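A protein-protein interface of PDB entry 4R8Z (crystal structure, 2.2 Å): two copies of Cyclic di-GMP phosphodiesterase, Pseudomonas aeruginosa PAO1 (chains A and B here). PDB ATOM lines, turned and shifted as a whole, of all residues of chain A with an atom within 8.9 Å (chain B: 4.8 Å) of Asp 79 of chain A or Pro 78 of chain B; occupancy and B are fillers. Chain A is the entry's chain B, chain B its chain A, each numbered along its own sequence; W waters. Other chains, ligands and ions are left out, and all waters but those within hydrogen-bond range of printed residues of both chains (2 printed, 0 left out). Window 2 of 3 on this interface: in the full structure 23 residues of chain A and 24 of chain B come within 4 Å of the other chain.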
ATOM      1  N   LEU A  22      -5.956  26.495  28.206  1.00  0.00           N
ATOM      2  CA  LEU A  22      -4.962  27.485  27.929  1.00  0.00           C
ATOM      3  C   LEU A  22      -5.156  28.076  26.546  1.00  0.00           C
ATOM      4  O   LEU A  22      -4.965  29.270  26.341  1.00  0.00           O
ATOM      5  CB  LEU A  22      -3.591  26.857  28.036  1.00  0.00           C
ATOM      6  CG  LEU A  22      -2.466  27.849  27.905  1.00  0.00           C
ATOM      7  CD1 LEU A  22      -2.256  28.550  29.235  1.00  0.00           C
ATOM      8  CD2 LEU A  22      -1.191  27.168  27.471  1.00  0.00           C
ATOM      9  N   ARG A  23      -5.603  27.274  25.595  1.00  0.00           N
ATOM     10  CA  ARG A  23      -5.652  27.767  24.229  1.00  0.00           C
ATOM     11  C   ARG A  23      -6.763  28.765  23.983  1.00  0.00           C
ATOM     12  O   ARG A  23      -6.604  29.672  23.172  1.00  0.00           O
ATOM     13  CB  ARG A  23      -5.794  26.608  23.254  1.00  0.00           C
ATOM     14  CG  ARG A  23      -4.463  25.925  22.986  1.00  0.00           C
ATOM     15  CD  ARG A  23      -4.652  24.555  22.328  1.00  0.00           C
ATOM     16  NE  ARG A  23      -5.003  24.635  20.925  1.00  0.00           N
ATOM     17  CZ  ARG A  23      -6.042  24.051  20.349  1.00  0.00           C
ATOM     18  NH1 ARG A  23      -6.885  23.314  21.050  1.00  0.00           N
ATOM     19  NH2 ARG A  23      -6.225  24.209  19.044  1.00  0.00           N
ATOM     20  N   ASP A  24      -7.928  28.559  24.599  1.00  0.00           N
ATOM     21  CA  ASP A  24      -9.054  29.469  24.341  1.00  0.00           C
ATOM     22  C   ASP A  24      -9.560  30.255  25.542  1.00  0.00           C
ATOM     23  O   ASP A  24     -10.471  31.043  25.386  1.00  0.00           O
ATOM     24  CB  ASP A  24     -10.251  28.754  23.712  1.00  0.00           C
ATOM     25  CG  ASP A  24     -11.067  27.923  24.726  1.00  0.00           C
ATOM     26  OD1 ASP A  24     -10.479  27.447  25.728  1.00  0.00           O
ATOM     27  OD2 ASP A  24     -12.287  27.748  24.495  1.00  0.00           O
ATOM     28  N   LYS A  74     -11.206  20.160  23.854  1.00  0.00           N
ATOM     29  CA  LYS A  74     -10.987  21.247  22.935  1.00  0.00           C
ATOM     30  C   LYS A  74      -9.694  21.171  22.199  1.00  0.00           C
ATOM     31  O   LYS A  74      -9.538  21.860  21.180  1.00  0.00           O
ATOM     32  CB  LYS A  74     -11.072  22.587  23.615  1.00  0.00           C
ATOM     33  CG  LYS A  74     -12.496  23.060  23.628  1.00  0.00           C
ATOM     34  CD  LYS A  74     -12.699  24.241  24.492  1.00  0.00           C
ATOM     35  CE  LYS A  74     -14.137  24.736  24.381  1.00  0.00           C
ATOM     36  NZ  LYS A  74     -14.338  25.707  25.515  1.00  0.00           N
ATOM     37  N   VAL A  75      -8.784  20.316  22.648  1.00  0.00           N
ATOM     38  CA  VAL A  75      -7.608  20.005  21.831  1.00  0.00           C
ATOM     39  C   VAL A  75      -7.928  19.407  20.460  1.00  0.00           C
ATOM     40  O   VAL A  75      -7.138  19.526  19.568  1.00  0.00           O
ATOM     41  CB  VAL A  75      -6.619  19.029  22.508  1.00  0.00           C
ATOM     42  CG1 VAL A  75      -5.871  19.694  23.656  1.00  0.00           C
ATOM     43  CG2 VAL A  75      -7.318  17.767  22.968  1.00  0.00           C
ATOM     44  N   ALA A  76      -9.072  18.779  20.297  1.00  0.00           N
ATOM     45  CA  ALA A  76      -9.538  18.355  18.926  1.00  0.00           C
ATOM     46  C   ALA A  76     -10.028  19.506  18.025  1.00  0.00           C
ATOM     47  O   ALA A  76     -10.449  19.287  16.916  1.00  0.00           O
ATOM     48  CB  ALA A  76     -10.627  17.289  19.021  1.00  0.00           C
ATOM     49  N   VAL A  77     -10.007  20.730  18.515  1.00  0.00           N
ATOM     50  CA  VAL A  77     -10.478  21.853  17.738  1.00  0.00           C
ATOM     51  C   VAL A  77      -9.258  22.654  17.332  1.00  0.00           C
ATOM     52  O   VAL A  77      -8.523  23.120  18.171  1.00  0.00           O
ATOM     53  CB  VAL A  77     -11.450  22.729  18.532  1.00  0.00           C
ATOM     54  CG1 VAL A  77     -12.150  23.763  17.625  1.00  0.00           C
ATOM     55  CG2 VAL A  77     -12.507  21.853  19.187  1.00  0.00           C
ATOM     56  N   PRO A  78      -9.046  22.813  16.021  1.00  0.00           N
ATOM     57  CA  PRO A  78      -7.954  23.641  15.492  1.00  0.00           C
ATOM     58  C   PRO A  78      -7.998  25.126  15.878  1.00  0.00           C
ATOM     59  O   PRO A  78      -9.085  25.697  16.059  1.00  0.00           O
ATOM     60  CB  PRO A  78      -8.080  23.515  13.964  1.00  0.00           C
ATOM     61  CG  PRO A  78      -9.199  22.559  13.681  1.00  0.00           C
ATOM     62  CD  PRO A  78      -9.876  22.176  14.971  1.00  0.00           C
ATOM     63  N   ASP A  79      -6.820  25.728  15.957  1.00  0.00           N
ATOM     64  CA  ASP A  79      -6.669  27.092  16.418  1.00  0.00           C
ATOM     65  C   ASP A  79      -7.583  28.007  15.607  1.00  0.00           C
ATOM     66  O   ASP A  79      -8.225  28.877  16.171  1.00  0.00           O
ATOM     67  CB  ASP A  79      -5.218  27.576  16.255  1.00  0.00           C
ATOM     68  CG  ASP A  79      -4.276  27.041  17.352  1.00  0.00           C
ATOM     69  OD1 ASP A  79      -4.582  26.012  18.027  1.00  0.00           O
ATOM     70  OD2 ASP A  79      -3.193  27.641  17.531  1.00  0.00           O
ATOM     71  N   ARG A  80      -7.626  27.794  14.299  1.00  0.00           N
ATOM     72  CA  ARG A  80      -8.318  28.701  13.395  1.00  0.00           C
ATOM     73  C   ARG A  80      -9.827  28.723  13.696  1.00  0.00           C
ATOM     74  O   ARG A  80     -10.452  29.774  13.587  1.00  0.00           O
ATOM     75  CB  ARG A  80      -8.016  28.322  11.947  1.00  0.00           C
ATOM     76  CG  ARG A  80      -8.737  27.094  11.494  1.00  0.00           C
ATOM     77  CD  ARG A  80      -8.239  26.502  10.171  1.00  0.00           C
ATOM     78  NE  ARG A  80      -9.050  25.315   9.870  1.00  0.00           N
ATOM     79  CZ  ARG A  80     -10.345  25.383   9.515  1.00  0.00           C
ATOM     80  NH1 ARG A  80     -11.047  24.273   9.296  1.00  0.00           N
ATOM     81  NH2 ARG A  80     -10.957  26.571   9.380  1.00  0.00           N
ATOM     82  N   VAL A  81     -10.390  27.605  14.180  1.00  0.00           N
ATOM     83  CA  VAL A  81     -11.775  27.599  14.623  1.00  0.00           C
ATOM     84  C   VAL A  81     -11.986  28.167  16.018  1.00  0.00           C
ATOM     85  O   VAL A  81     -12.881  28.971  16.277  1.00  0.00           O
ATOM     86  CB  VAL A  81     -12.364  26.212  14.552  1.00  0.00           C
ATOM     87  CG1 VAL A  81     -13.730  26.199  15.202  1.00  0.00           C
ATOM     88  CG2 VAL A  81     -12.466  25.762  13.121  1.00  0.00           C
ATOM     89  N   LEU A  82     -11.126  27.752  16.913  1.00  0.00           N
ATOM     90  CA  LEU A  82     -11.301  27.995  18.322  1.00  0.00           C
ATOM     91  C   LEU A  82     -11.053  29.430  18.652  1.00  0.00           C
ATOM     92  O   LEU A  82     -11.672  29.964  19.571  1.00  0.00           O
ATOM     93  CB  LEU A  82     -10.299  27.102  19.053  1.00  0.00           C
ATOM     94  CG  LEU A  82     -10.442  26.894  20.524  1.00  0.00           C
ATOM     95  CD1 LEU A  82     -11.719  26.144  20.804  1.00  0.00           C
ATOM     96  CD2 LEU A  82      -9.237  26.092  21.006  1.00  0.00           C
ATOM     97  N   LEU A  83     -10.137  30.048  17.899  1.00  0.00           N
ATOM     98  CA  LEU A  83      -9.777  31.462  18.059  1.00  0.00           C
ATOM     99  C   LEU A  83     -10.537  32.427  17.112  1.00  0.00           C
ATOM    100  O   LEU A  83     -10.240  33.618  17.074  1.00  0.00           O
ATOM    101  CB  LEU A  83      -8.255  31.616  17.853  1.00  0.00           C
ATOM    102  CG  LEU A  83      -7.315  30.791  18.765  1.00  0.00           C
ATOM    103  CD1 LEU A  83      -5.856  31.252  18.677  1.00  0.00           C
ATOM    104  CD2 LEU A  83      -7.784  30.808  20.226  1.00  0.00           C
ATOM    105  N   ASN A  84     -11.506  31.921  16.349  1.00  0.00           N
ATOM    106  CA  ASN A  84     -12.314  32.753  15.445  1.00  0.00           C
ATOM    107  C   ASN A  84     -13.459  33.454  16.179  1.00  0.00           C
ATOM    108  O   ASN A  84     -14.379  32.784  16.634  1.00  0.00           O
ATOM    109  CB  ASN A  84     -12.889  31.867  14.332  1.00  0.00           C
ATOM    110  CG  ASN A  84     -13.594  32.654  13.229  1.00  0.00           C
ATOM    111  OD1 ASN A  84     -14.173  33.711  13.448  1.00  0.00           O
ATOM    112  ND2 ASN A  84     -13.551  32.118  12.036  1.00  0.00           N
ATOM    113  N   PRO A  85     -13.434  34.804  16.263  1.00  0.00           N
ATOM    114  CA  PRO A  85     -14.494  35.486  17.037  1.00  0.00           C
ATOM    115  C   PRO A  85     -15.844  35.620  16.285  1.00  0.00           C
ATOM    116  O   PRO A  85     -16.871  35.824  16.923  1.00  0.00           O
ATOM    117  CB  PRO A  85     -13.884  36.869  17.306  1.00  0.00           C
ATOM    118  CG  PRO A  85     -13.012  37.122  16.107  1.00  0.00           C
ATOM    119  CD  PRO A  85     -12.578  35.780  15.548  1.00  0.00           C
ATOM    120  N   ASP A  92     -16.953  24.169  10.267  1.00  0.00           N
ATOM    121  CA  ASP A  92     -16.189  24.655  11.396  1.00  0.00           C
ATOM    122  C   ASP A  92     -16.991  24.535  12.700  1.00  0.00           C
ATOM    123  O   ASP A  92     -16.446  24.204  13.752  1.00  0.00           O
ATOM    124  CB  ASP A  92     -15.746  26.104  11.168  1.00  0.00           C
ATOM    125  CG  ASP A  92     -14.590  26.209  10.127  1.00  0.00           C
ATOM    126  OD1 ASP A  92     -14.087  25.141   9.647  1.00  0.00           O
ATOM    127  OD2 ASP A  92     -14.187  27.360   9.768  1.00  0.00           O
ATOM    128  N   LEU A  95     -16.622  21.105  13.786  1.00  0.00           N
ATOM    129  CA  LEU A  95     -15.336  20.914  14.477  1.00  0.00           C
ATOM    130  C   LEU A  95     -15.335  21.463  15.923  1.00  0.00           C
ATOM    131  O   LEU A  95     -14.905  20.785  16.825  1.00  0.00           O
ATOM    132  CB  LEU A  95     -14.197  21.560  13.699  1.00  0.00           C
ATOM    133  CG  LEU A  95     -13.794  20.802  12.422  1.00  0.00           C
ATOM    134  CD1 LEU A  95     -12.728  21.612  11.697  1.00  0.00           C
ATOM    135  CD2 LEU A  95     -13.227  19.408  12.695  1.00  0.00           C
ATOM    136  N   LEU A  96     -15.867  22.652  16.143  1.00  0.00           N
ATOM    137  CA  LEU A  96     -16.069  23.190  17.485  1.00  0.00           C
ATOM    138  C   LEU A  96     -16.932  22.271  18.393  1.00  0.00           C
ATOM    139  O   LEU A  96     -16.542  21.958  19.535  1.00  0.00           O
ATOM    140  CB  LEU A  96     -16.631  24.595  17.401  1.00  0.00           C
ATOM    141  CG  LEU A  96     -16.917  25.335  18.727  1.00  0.00           C
ATOM    142  CD1 LEU A  96     -15.646  25.547  19.495  1.00  0.00           C
ATOM    143  CD2 LEU A  96     -17.648  26.673  18.527  1.00  0.00           C
ATOM    144  N   ARG B  23      -2.945  16.651  19.184  1.00  0.00           N
ATOM    145  CA  ARG B  23      -2.713  17.665  18.184  1.00  0.00           C
ATOM    146  C   ARG B  23      -1.482  17.381  17.313  1.00  0.00           C
ATOM    147  O   ARG B  23      -1.508  17.666  16.121  1.00  0.00           O
ATOM    148  CB  ARG B  23      -2.545  19.035  18.825  1.00  0.00           C
ATOM    149  CG  ARG B  23      -3.884  19.656  19.139  1.00  0.00           C
ATOM    150  CD  ARG B  23      -3.788  20.840  20.100  1.00  0.00           C
ATOM    151  NE  ARG B  23      -3.302  22.053  19.454  1.00  0.00           N
ATOM    152  CZ  ARG B  23      -2.238  22.758  19.846  1.00  0.00           C
ATOM    153  NH1 ARG B  23      -1.505  22.409  20.903  1.00  0.00           N
ATOM    154  NH2 ARG B  23      -1.866  23.825  19.149  1.00  0.00           N
ATOM    155  N   ALA B  76       0.532  24.998  24.864  1.00  0.00           N
ATOM    156  CA  ALA B  76       1.072  26.368  24.717  1.00  0.00           C
ATOM    157  C   ALA B  76       1.714  26.644  23.340  1.00  0.00           C
ATOM    158  O   ALA B  76       2.201  27.750  23.080  1.00  0.00           O
ATOM    159  CB  ALA B  76       2.073  26.687  25.824  1.00  0.00           C
ATOM    160  N   VAL B  77       1.692  25.681  22.445  1.00  0.00           N
ATOM    161  CA  VAL B  77       2.296  25.874  21.153  1.00  0.00           C
ATOM    162  C   VAL B  77       1.177  25.953  20.151  1.00  0.00           C
ATOM    163  O   VAL B  77       0.364  25.001  20.035  1.00  0.00           O
ATOM    164  CB  VAL B  77       3.239  24.709  20.796  1.00  0.00           C
ATOM    165  CG1 VAL B  77       4.045  25.045  19.552  1.00  0.00           C
ATOM    166  CG2 VAL B  77       4.193  24.428  21.953  1.00  0.00           C
ATOM    167  N   PRO B  78       1.100  27.070  19.406  1.00  0.00           N
ATOM    168  CA  PRO B  78       0.079  27.234  18.347  1.00  0.00           C
ATOM    169  C   PRO B  78       0.171  26.263  17.211  1.00  0.00           C
ATOM    170  O   PRO B  78       1.256  25.808  16.850  1.00  0.00           O
ATOM    171  CB  PRO B  78       0.292  28.673  17.811  1.00  0.00           C
ATOM    172  CG  PRO B  78       1.356  29.287  18.660  1.00  0.00           C
ATOM    173  CD  PRO B  78       1.911  28.278  19.620  1.00  0.00           C
ATOM    174  N   ASP B  79      -0.981  25.956  16.648  1.00  0.00           N
ATOM    175  CA  ASP B  79      -1.093  24.952  15.580  1.00  0.00           C
ATOM    176  C   ASP B  79      -0.063  25.222  14.485  1.00  0.00           C
ATOM    177  O   ASP B  79       0.574  24.311  14.026  1.00  0.00           O
ATOM    178  CB  ASP B  79      -2.494  24.985  14.931  1.00  0.00           C
ATOM    179  CG  ASP B  79      -3.601  24.364  15.809  1.00  0.00           C
ATOM    180  OD1 ASP B  79      -3.378  24.118  17.021  1.00  0.00           O
ATOM    181  OD2 ASP B  79      -4.735  24.151  15.276  1.00  0.00           O
ATOM    182  N   ARG B  80       0.071  26.486  14.085  1.00  0.00           N
ATOM    183  CA  ARG B  80       0.895  26.838  12.936  1.00  0.00           C
ATOM    184  C   ARG B  80       2.359  26.471  13.172  1.00  0.00           C
ATOM    185  O   ARG B  80       3.026  26.099  12.254  1.00  0.00           O
ATOM    186  CB  ARG B  80       0.767  28.337  12.573  1.00  0.00           C
ATOM    187  CG  ARG B  80       1.780  29.230  13.231  1.00  0.00           C
ATOM    188  CD  ARG B  80       1.454  30.709  13.118  1.00  0.00           C
ATOM    189  NE  ARG B  80       2.505  31.449  13.827  1.00  0.00           N
ATOM    190  CZ  ARG B  80       2.340  32.046  15.013  1.00  0.00           C
ATOM    191  NH1 ARG B  80       1.167  32.037  15.661  1.00  0.00           N
ATOM    192  NH2 ARG B  80       3.363  32.651  15.572  1.00  0.00           N
ATOM    193  N   VAL B  81       2.836  26.573  14.406  1.00  0.00           N
ATOM    194  CA  VAL B  81       4.185  26.146  14.744  1.00  0.00           C
ATOM    195  C   VAL B  81       4.289  24.637  14.907  1.00  0.00           C
ATOM    196  O   VAL B  81       5.186  24.006  14.393  1.00  0.00           O
ATOM    197  CB  VAL B  81       4.657  26.795  16.025  1.00  0.00           C
ATOM    198  CG1 VAL B  81       5.957  26.156  16.482  1.00  0.00           C
ATOM    199  CG2 VAL B  81       4.834  28.272  15.804  1.00  0.00           C
ATOM    200  N   LEU B  82       3.338  24.056  15.608  1.00  0.00           N
ATOM    201  CA  LEU B  82       3.416  22.656  16.001  1.00  0.00           C
ATOM    202  C   LEU B  82       3.233  21.745  14.830  1.00  0.00           C
ATOM    203  O   LEU B  82       3.770  20.649  14.815  1.00  0.00           O
ATOM    204  CB  LEU B  82       2.294  22.391  17.028  1.00  0.00           C
ATOM    205  CG  LEU B  82       2.324  21.128  17.851  1.00  0.00           C
ATOM    206  CD1 LEU B  82       3.545  21.139  18.741  1.00  0.00           C
ATOM    207  CD2 LEU B  82       1.060  21.109  18.691  1.00  0.00           C
ATOM    208  N   LEU B  95       8.567  29.496  20.614  1.00  0.00           N
ATOM    209  CA  LEU B  95       7.233  29.029  20.986  1.00  0.00           C
ATOM    210  C   LEU B  95       7.176  27.497  21.166  1.00  0.00           C
ATOM    211  O   LEU B  95       6.589  27.005  22.121  1.00  0.00           O
ATOM    212  CB  LEU B  95       6.216  29.498  19.979  1.00  0.00           C
ATOM    213  CG  LEU B  95       5.847  31.001  20.087  1.00  0.00           C
ATOM    214  CD1 LEU B  95       4.906  31.365  18.961  1.00  0.00           C
ATOM    215  CD2 LEU B  95       5.148  31.369  21.381  1.00  0.00           C
HETATM  216  O   HOH W   1      -2.046  28.659  14.961  1.00  0.00           O
HETATM  217  O   HOH W   2      -5.572  25.984  12.987  1.00  0.00           O
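The side-chain carboxylate of Asp 79 of chain A is in salt-bridge range of the guanidinium group of Arg 23 of chain B. NH2 of Arg 23 of chain A lies within salt-bridge range of OD1 of Asp 79 of chain B (3.5 Å). OD2 of Asp 79 of chain B lies within hydrogen-bond range of N of Asp 79 of chain A, 2.7 Å away. The guanidinium group (NE) of Arg 23 of chain A lies close to the guanidinium group (NE) of Arg 23 of chain B (3.4 Å).
NH2 of Arg 23 of chain B is in hydrogen-bond range of O of Val 77 of chain B. The side-chain carboxylate (OD1) of Asp 79 of chain B is in salt-bridge range of the guanidinium group (NH2) of Arg 23 of chain B, at 2.6 Å. O of Lys 74 of chain A is in hydrogen-bond range of NH1 of Arg 23 of chain A (3.0 Å). The guanidinium group (NH2) of Arg 23 of chain A lies within hydrogen-bond range of the backbone carbonyl oxygen (O) of Val 77 of chain A (2.7 Å). The guanidinium group (NH2) of Arg 23 of chain A lies within salt-bridge range of the side-chain carboxylate (OD1) of Asp 79 of chain A.
Among the printed residues, pairs that only touch across the chains: Pro 78 of chain A with Asp 79 of chain B (3.3 Å), Val 75 of chain A with Arg 23 of chain B (3.3 Å), Asp 79 of chain A with Pro 78 of chain B (3.4 Å) and Leu 22 of chain A with Ala 76 of chain B (3.7 Å).
Of the printed residues of chain B, Leu 22 of chain A touches Ala 76. Asp 24 of chain A touches none of the printed residues of chain B. Of the printed residues of chain B, Val 75 of chain A touches Arg 23 (3.3 Å). Of the printed residues of chain B, Pro 78 of chain A touches Asp 79. Asp 79 of chain A touches three residues of chain B. Asp 92 of chain A touches none of the printed residues of chain B. Of the printed residues of chain A, Arg 23 of chain B touches Arg 23, Val 75 and Asp 79. Printed residues of chain A within 4 Å of Ala 76 of chain B: Leu 22 (3.7 Å). No residue of chain A comes within 4 Å of Val 77 of chain B. Printed residues of chain A within 4 Å of Pro 78 of chain B: Asp 79 (3.4 Å). Printed residues of chain A within 4 Å of Asp 79 of chain B: Arg 23, Pro 78 and Asp 79. The nearest printed residue of chain B that does not touch Asp 79 of chain A is Arg 80 of chain B (4.9 Å).
Of the 9 printed residues of chain B, 4 touch a printed residue of chain A. Hydrophobic or aromatic side chains of chain B that line the printed part of chain A: Ala 76 and Pro 78. Among the printed residues, 8 pairs touch across the chains.
Arg 23 of chain B touches its own counterpart, Arg 23 of chain A. Arg 23 of chain A touches Asp 79 of chain B, and with the chains exchanged Asp 79 of chain A touches Arg 23 of chain B. Pro 78 of chain A touches Asp 79 of chain B, and with the chains exchanged Asp 79 of chain A touches Pro 78 of chain B. Asp 79 of chain A touches its own counterpart, Asp 79 of chain B. 9 positions are printed for both chains. Of the 8 pairs that touch across the chains among the printed residues, 6 have their exchanged pair printed and touching as well.
Water W1 lies within hydrogen-bond range of the side-chain carboxylate (OD2) of Asp 79 of chain A, the backbone NH (N) of Arg 80 of chain B and the backbone NH (N) of Asp 79 of chain B. Water W2 lies within hydrogen-bond range of N of Arg 80 of chain A (3.0 Å), OD2 of Asp 79 of chain B (3.0 Å) and N of Asp 79 of chain A (3.2 Å).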
